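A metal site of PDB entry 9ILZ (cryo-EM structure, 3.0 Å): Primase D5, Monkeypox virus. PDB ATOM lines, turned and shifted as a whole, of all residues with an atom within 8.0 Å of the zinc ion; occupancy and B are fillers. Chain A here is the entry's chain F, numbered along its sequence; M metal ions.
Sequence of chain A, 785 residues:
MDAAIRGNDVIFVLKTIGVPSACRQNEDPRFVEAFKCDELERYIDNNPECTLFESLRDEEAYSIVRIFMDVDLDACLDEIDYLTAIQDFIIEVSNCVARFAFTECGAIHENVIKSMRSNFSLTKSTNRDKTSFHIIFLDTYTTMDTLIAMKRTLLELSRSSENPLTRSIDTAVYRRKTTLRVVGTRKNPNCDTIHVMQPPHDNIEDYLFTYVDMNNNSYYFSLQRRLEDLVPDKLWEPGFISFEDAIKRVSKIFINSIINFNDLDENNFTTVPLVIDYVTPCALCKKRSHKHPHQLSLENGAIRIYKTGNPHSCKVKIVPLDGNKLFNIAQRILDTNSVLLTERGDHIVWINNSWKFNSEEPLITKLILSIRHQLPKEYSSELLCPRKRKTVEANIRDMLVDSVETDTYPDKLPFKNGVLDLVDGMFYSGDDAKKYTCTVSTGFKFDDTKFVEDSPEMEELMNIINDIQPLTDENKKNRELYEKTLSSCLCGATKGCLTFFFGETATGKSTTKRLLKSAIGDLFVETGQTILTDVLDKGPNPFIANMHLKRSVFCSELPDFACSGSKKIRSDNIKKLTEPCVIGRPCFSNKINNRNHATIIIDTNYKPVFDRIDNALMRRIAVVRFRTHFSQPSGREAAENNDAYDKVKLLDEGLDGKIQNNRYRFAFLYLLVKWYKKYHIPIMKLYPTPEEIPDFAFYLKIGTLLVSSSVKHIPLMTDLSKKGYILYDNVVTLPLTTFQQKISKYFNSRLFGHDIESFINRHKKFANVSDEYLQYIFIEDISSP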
ATOM      1  N   PHE A 254     -12.553 -12.062 -14.624  1.00  0.00           N
ATOM      2  CA  PHE A 254     -11.257 -11.930 -13.992  1.00  0.00           C
ATOM      3  C   PHE A 254     -11.451 -11.779 -12.489  1.00  0.00           C
ATOM      4  O   PHE A 254     -11.927 -10.746 -12.012  1.00  0.00           O
ATOM      5  CB  PHE A 254     -10.502 -10.729 -14.559  1.00  0.00           C
ATOM      6  CG  PHE A 254      -9.685 -11.047 -15.787  1.00  0.00           C
ATOM      7  CD1 PHE A 254      -8.865 -12.152 -15.818  1.00  0.00           C
ATOM      8  CD2 PHE A 254      -9.750 -10.231 -16.905  1.00  0.00           C
ATOM      9  CE1 PHE A 254      -8.113 -12.454 -16.935  1.00  0.00           C
ATOM     10  CE2 PHE A 254      -9.012 -10.525 -18.031  1.00  0.00           C
ATOM     11  CZ  PHE A 254      -8.189 -11.631 -18.042  1.00  0.00           C
ATOM     12  N   PRO A 281      -4.095 -16.375  -8.508  1.00  0.00           N
ATOM     13  CA  PRO A 281      -3.879 -16.860  -9.878  1.00  0.00           C
ATOM     14  C   PRO A 281      -5.122 -16.672 -10.745  1.00  0.00           C
ATOM     15  O   PRO A 281      -6.251 -16.767 -10.268  1.00  0.00           O
ATOM     16  CB  PRO A 281      -3.547 -18.340  -9.677  1.00  0.00           C
ATOM     17  CG  PRO A 281      -3.951 -18.652  -8.264  1.00  0.00           C
ATOM     18  CD  PRO A 281      -3.733 -17.391  -7.505  1.00  0.00           C
ATOM     19  N   CYS A 282      -4.889 -16.396 -12.024  1.00  0.00           N
ATOM     20  CA  CYS A 282      -5.980 -16.108 -12.939  1.00  0.00           C
ATOM     21  C   CYS A 282      -6.883 -17.320 -13.119  1.00  0.00           C
ATOM     22  O   CYS A 282      -6.457 -18.467 -12.964  1.00  0.00           O
ATOM     23  CB  CYS A 282      -5.433 -15.652 -14.299  1.00  0.00           C
ATOM     24  SG  CYS A 282      -4.529 -16.911 -15.241  1.00  0.00           S
ATOM     25  N   ALA A 283      -8.150 -17.055 -13.435  1.00  0.00           N
ATOM     26  CA  ALA A 283      -9.139 -18.119 -13.530  1.00  0.00           C
ATOM     27  C   ALA A 283      -8.923 -18.999 -14.755  1.00  0.00           C
ATOM     28  O   ALA A 283      -9.311 -20.165 -14.752  1.00  0.00           O
ATOM     29  CB  ALA A 283     -10.548 -17.527 -13.538  1.00  0.00           C
ATOM     30  N   LEU A 284      -8.311 -18.448 -15.809  1.00  0.00           N
ATOM     31  CA  LEU A 284      -8.104 -19.225 -17.032  1.00  0.00           C
ATOM     32  C   LEU A 284      -7.190 -20.413 -16.774  1.00  0.00           C
ATOM     33  O   LEU A 284      -7.593 -21.574 -16.950  1.00  0.00           O
ATOM     34  CB  LEU A 284      -7.516 -18.325 -18.117  1.00  0.00           C
ATOM     35  CG  LEU A 284      -8.160 -16.949 -18.288  1.00  0.00           C
ATOM     36  CD1 LEU A 284      -7.490 -16.168 -19.416  1.00  0.00           C
ATOM     37  CD2 LEU A 284      -9.659 -17.078 -18.539  1.00  0.00           C
ATOM     38  N   CYS A 285      -5.968 -20.156 -16.341  1.00  0.00           N
ATOM     39  CA  CYS A 285      -5.003 -21.198 -16.007  1.00  0.00           C
ATOM     40  C   CYS A 285      -4.490 -20.952 -14.589  1.00  0.00           C
ATOM     41  O   CYS A 285      -4.383 -19.809 -14.150  1.00  0.00           O
ATOM     42  CB  CYS A 285      -3.836 -21.209 -16.995  1.00  0.00           C
ATOM     43  SG  CYS A 285      -2.588 -19.935 -16.690  1.00  0.00           S
ATOM     44  N   LYS A 286      -4.177 -22.038 -13.883  1.00  0.00           N
ATOM     45  CA  LYS A 286      -3.700 -21.904 -12.513  1.00  0.00           C
ATOM     46  C   LYS A 286      -2.384 -21.126 -12.498  1.00  0.00           C
ATOM     47  O   LYS A 286      -2.359 -19.964 -12.078  1.00  0.00           O
ATOM     48  CB  LYS A 286      -3.541 -23.282 -11.872  1.00  0.00           C
ATOM     49  CG  LYS A 286      -2.748 -23.355 -10.568  1.00  0.00           C
ATOM     50  CD  LYS A 286      -3.098 -22.262  -9.563  1.00  0.00           C
ATOM     51  CE  LYS A 286      -2.127 -22.286  -8.394  1.00  0.00           C
ATOM     52  NZ  LYS A 286      -1.671 -20.925  -7.999  1.00  0.00           N
ATOM     53  N   LYS A 287      -1.310 -21.744 -13.009  1.00  0.00           N
ATOM     54  CA  LYS A 287       0.005 -21.126 -13.129  1.00  0.00           C
ATOM     55  C   LYS A 287       0.350 -20.292 -11.900  1.00  0.00           C
ATOM     56  O   LYS A 287       0.016 -20.683 -10.770  1.00  0.00           O
ATOM     57  CB  LYS A 287       0.065 -20.265 -14.394  1.00  0.00           C
ATOM     58  CG  LYS A 287       1.417 -20.248 -15.104  1.00  0.00           C
ATOM     59  CD  LYS A 287       2.032 -18.859 -15.114  1.00  0.00           C
ATOM     60  CE  LYS A 287       3.328 -18.832 -15.917  1.00  0.00           C
ATOM     61  NZ  LYS A 287       3.933 -17.478 -15.927  1.00  0.00           N
ATOM     62  N   ARG A 288       1.028 -19.166 -12.105  1.00  0.00           N
ATOM     63  CA  ARG A 288       1.164 -18.120 -11.096  1.00  0.00           C
ATOM     64  C   ARG A 288       1.774 -16.875 -11.714  1.00  0.00           C
ATOM     65  O   ARG A 288       2.816 -16.952 -12.363  1.00  0.00           O
ATOM     66  CB  ARG A 288       2.020 -18.595  -9.909  1.00  0.00           C
ATOM     67  CG  ARG A 288       2.378 -17.493  -8.930  1.00  0.00           C
ATOM     68  CD  ARG A 288       1.178 -17.109  -8.072  1.00  0.00           C
ATOM     69  NE  ARG A 288       0.476 -15.938  -8.592  1.00  0.00           N
ATOM     70  CZ  ARG A 288      -0.483 -15.294  -7.945  1.00  0.00           C
ATOM     71  NH1 ARG A 288      -0.886 -15.668  -6.745  1.00  0.00           N
ATOM     72  NH2 ARG A 288      -1.063 -14.241  -8.524  1.00  0.00           N
ATOM     73  N   SER A 289       1.129 -15.718 -11.515  1.00  0.00           N
ATOM     74  CA  SER A 289       1.704 -14.415 -11.864  1.00  0.00           C
ATOM     75  C   SER A 289       2.077 -14.347 -13.347  1.00  0.00           C
ATOM     76  O   SER A 289       3.248 -14.318 -13.730  1.00  0.00           O
ATOM     77  CB  SER A 289       2.914 -14.092 -10.974  1.00  0.00           C
ATOM     78  OG  SER A 289       3.522 -12.882 -11.360  1.00  0.00           O
ATOM     79  N   HIS A 290       1.038 -14.372 -14.185  1.00  0.00           N
ATOM     80  CA  HIS A 290       1.231 -14.244 -15.622  1.00  0.00           C
ATOM     81  C   HIS A 290       2.077 -13.030 -15.950  1.00  0.00           C
ATOM     82  O   HIS A 290       1.838 -11.930 -15.434  1.00  0.00           O
ATOM     83  CB  HIS A 290      -0.123 -14.149 -16.334  1.00  0.00           C
ATOM     84  CG  HIS A 290      -0.959 -15.389 -16.230  1.00  0.00           C
ATOM     85  ND1 HIS A 290      -0.439 -16.605 -15.837  1.00  0.00           N
ATOM     86  CD2 HIS A 290      -2.274 -15.601 -16.467  1.00  0.00           C
ATOM     87  CE1 HIS A 290      -1.401 -17.511 -15.842  1.00  0.00           C
ATOM     88  NE2 HIS A 290      -2.519 -16.927 -16.224  1.00  0.00           N
ATOM     89  N   HIS A 294      -3.040  -9.206 -20.967  1.00  0.00           N
ATOM     90  CA  HIS A 294      -4.058  -9.852 -21.778  1.00  0.00           C
ATOM     91  C   HIS A 294      -4.634  -8.866 -22.792  1.00  0.00           C
ATOM     92  O   HIS A 294      -4.296  -7.673 -22.798  1.00  0.00           O
ATOM     93  CB  HIS A 294      -5.152 -10.450 -20.891  1.00  0.00           C
ATOM     94  CG  HIS A 294      -4.785 -11.765 -20.287  1.00  0.00           C
ATOM     95  ND1 HIS A 294      -3.680 -11.938 -19.483  1.00  0.00           N
ATOM     96  CD2 HIS A 294      -5.390 -12.979 -20.366  1.00  0.00           C
ATOM     97  CE1 HIS A 294      -3.612 -13.192 -19.089  1.00  0.00           C
ATOM     98  NE2 HIS A 294      -4.633 -13.845 -19.617  1.00  0.00           N
ATOM     99  N   LYS A 307      -4.046 -14.042 -24.142  1.00  0.00           N
ATOM    100  CA  LYS A 307      -2.861 -13.527 -23.478  1.00  0.00           C
ATOM    101  C   LYS A 307      -1.728 -13.400 -24.490  1.00  0.00           C
ATOM    102  O   LYS A 307      -1.408 -14.362 -25.196  1.00  0.00           O
ATOM    103  CB  LYS A 307      -2.439 -14.429 -22.320  1.00  0.00           C
ATOM    104  CG  LYS A 307      -1.238 -13.947 -21.538  1.00  0.00           C
ATOM    105  CD  LYS A 307      -0.011 -14.795 -21.811  1.00  0.00           C
ATOM    106  CE  LYS A 307       1.029 -14.660 -20.720  1.00  0.00           C
ATOM    107  NZ  LYS A 307       2.254 -15.466 -20.992  1.00  0.00           N
ATOM    108  N   HIS A 312      -0.116 -21.050 -25.346  1.00  0.00           N
ATOM    109  CA  HIS A 312      -0.477 -22.114 -24.426  1.00  0.00           C
ATOM    110  C   HIS A 312      -0.397 -21.695 -22.956  1.00  0.00           C
ATOM    111  O   HIS A 312      -0.784 -22.483 -22.089  1.00  0.00           O
ATOM    112  CB  HIS A 312       0.415 -23.334 -24.650  1.00  0.00           C
ATOM    113  CG  HIS A 312       0.280 -23.942 -26.015  1.00  0.00           C
ATOM    114  ND1 HIS A 312      -0.727 -24.832 -26.326  1.00  0.00           N
ATOM    115  CD2 HIS A 312       1.008 -23.781 -27.142  1.00  0.00           C
ATOM    116  CE1 HIS A 312      -0.604 -25.204 -27.591  1.00  0.00           C
ATOM    117  NE2 HIS A 312       0.445 -24.578 -28.108  1.00  0.00           N
ATOM    118  N   SER A 313       0.080 -20.488 -22.668  1.00  0.00           N
ATOM    119  CA  SER A 313       0.232 -20.064 -21.278  1.00  0.00           C
ATOM    120  C   SER A 313      -1.126 -19.903 -20.605  1.00  0.00           C
ATOM    121  O   SER A 313      -1.349 -20.436 -19.513  1.00  0.00           O
ATOM    122  CB  SER A 313       1.026 -18.751 -21.223  1.00  0.00           C
ATOM    123  OG  SER A 313       0.640 -17.886 -22.266  1.00  0.00           O
ATOM    124  N   CYS A 314      -2.044 -19.185 -21.234  1.00  0.00           N
ATOM    125  CA  CYS A 314      -3.363 -18.922 -20.675  1.00  0.00           C
ATOM    126  C   CYS A 314      -4.440 -19.496 -21.597  1.00  0.00           C
ATOM    127  O   CYS A 314      -4.285 -19.496 -22.820  1.00  0.00           O
ATOM    128  CB  CYS A 314      -3.602 -17.429 -20.465  1.00  0.00           C
ATOM    129  SG  CYS A 314      -3.093 -16.799 -18.849  1.00  0.00           S
ATOM    130  N   LYS A 315      -5.523 -19.970 -20.992  1.00  0.00           N
ATOM    131  CA  LYS A 315      -6.610 -20.577 -21.752  1.00  0.00           C
ATOM    132  C   LYS A 315      -7.462 -19.493 -22.414  1.00  0.00           C
ATOM    133  O   LYS A 315      -7.618 -18.390 -21.900  1.00  0.00           O
ATOM    134  CB  LYS A 315      -7.469 -21.452 -20.842  1.00  0.00           C
ATOM    135  CG  LYS A 315      -8.402 -22.391 -21.578  1.00  0.00           C
ATOM    136  CD  LYS A 315      -7.606 -23.406 -22.391  1.00  0.00           C
ATOM    137  CE  LYS A 315      -6.743 -24.281 -21.494  1.00  0.00           C
ATOM    138  NZ  LYS A 315      -7.562 -25.173 -20.630  1.00  0.00           N
ATOM    139  N   VAL A 316      -8.017 -19.839 -23.576  1.00  0.00           N
ATOM    140  CA  VAL A 316      -8.874 -18.919 -24.321  1.00  0.00           C
ATOM    141  C   VAL A 316     -10.282 -18.945 -23.734  1.00  0.00           C
ATOM    142  O   VAL A 316     -10.815 -20.006 -23.397  1.00  0.00           O
ATOM    143  CB  VAL A 316      -8.879 -19.284 -25.820  1.00  0.00           C
ATOM    144  CG1 VAL A 316      -9.214 -20.747 -26.011  1.00  0.00           C
ATOM    145  CG2 VAL A 316      -9.845 -18.395 -26.591  1.00  0.00           C
HETATM  146 ZN    ZN M   1      -3.957 -18.118 -17.137  1.00  0.00          ZN
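O of Ser 313 lies close to SG of Cys 285 (3.1 Å).
SG of Cys 314 sits close to NE2 of His 294 (3.4 Å).
Merely in contact with the zinc ion: Leu 284.
Within 4 Å of the zinc ion: Cys 282, Leu 284, Cys 285, His 290 and Cys 314.
The zinc ion is bound by NE2 of His 290 (2.1 Å), SG of Cys 282 (2.3 Å), SG of Cys 285 (2.3 Å) and SG of Cys 314 (2.3 Å).
The zinc ion has four donor atoms within binding distance.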
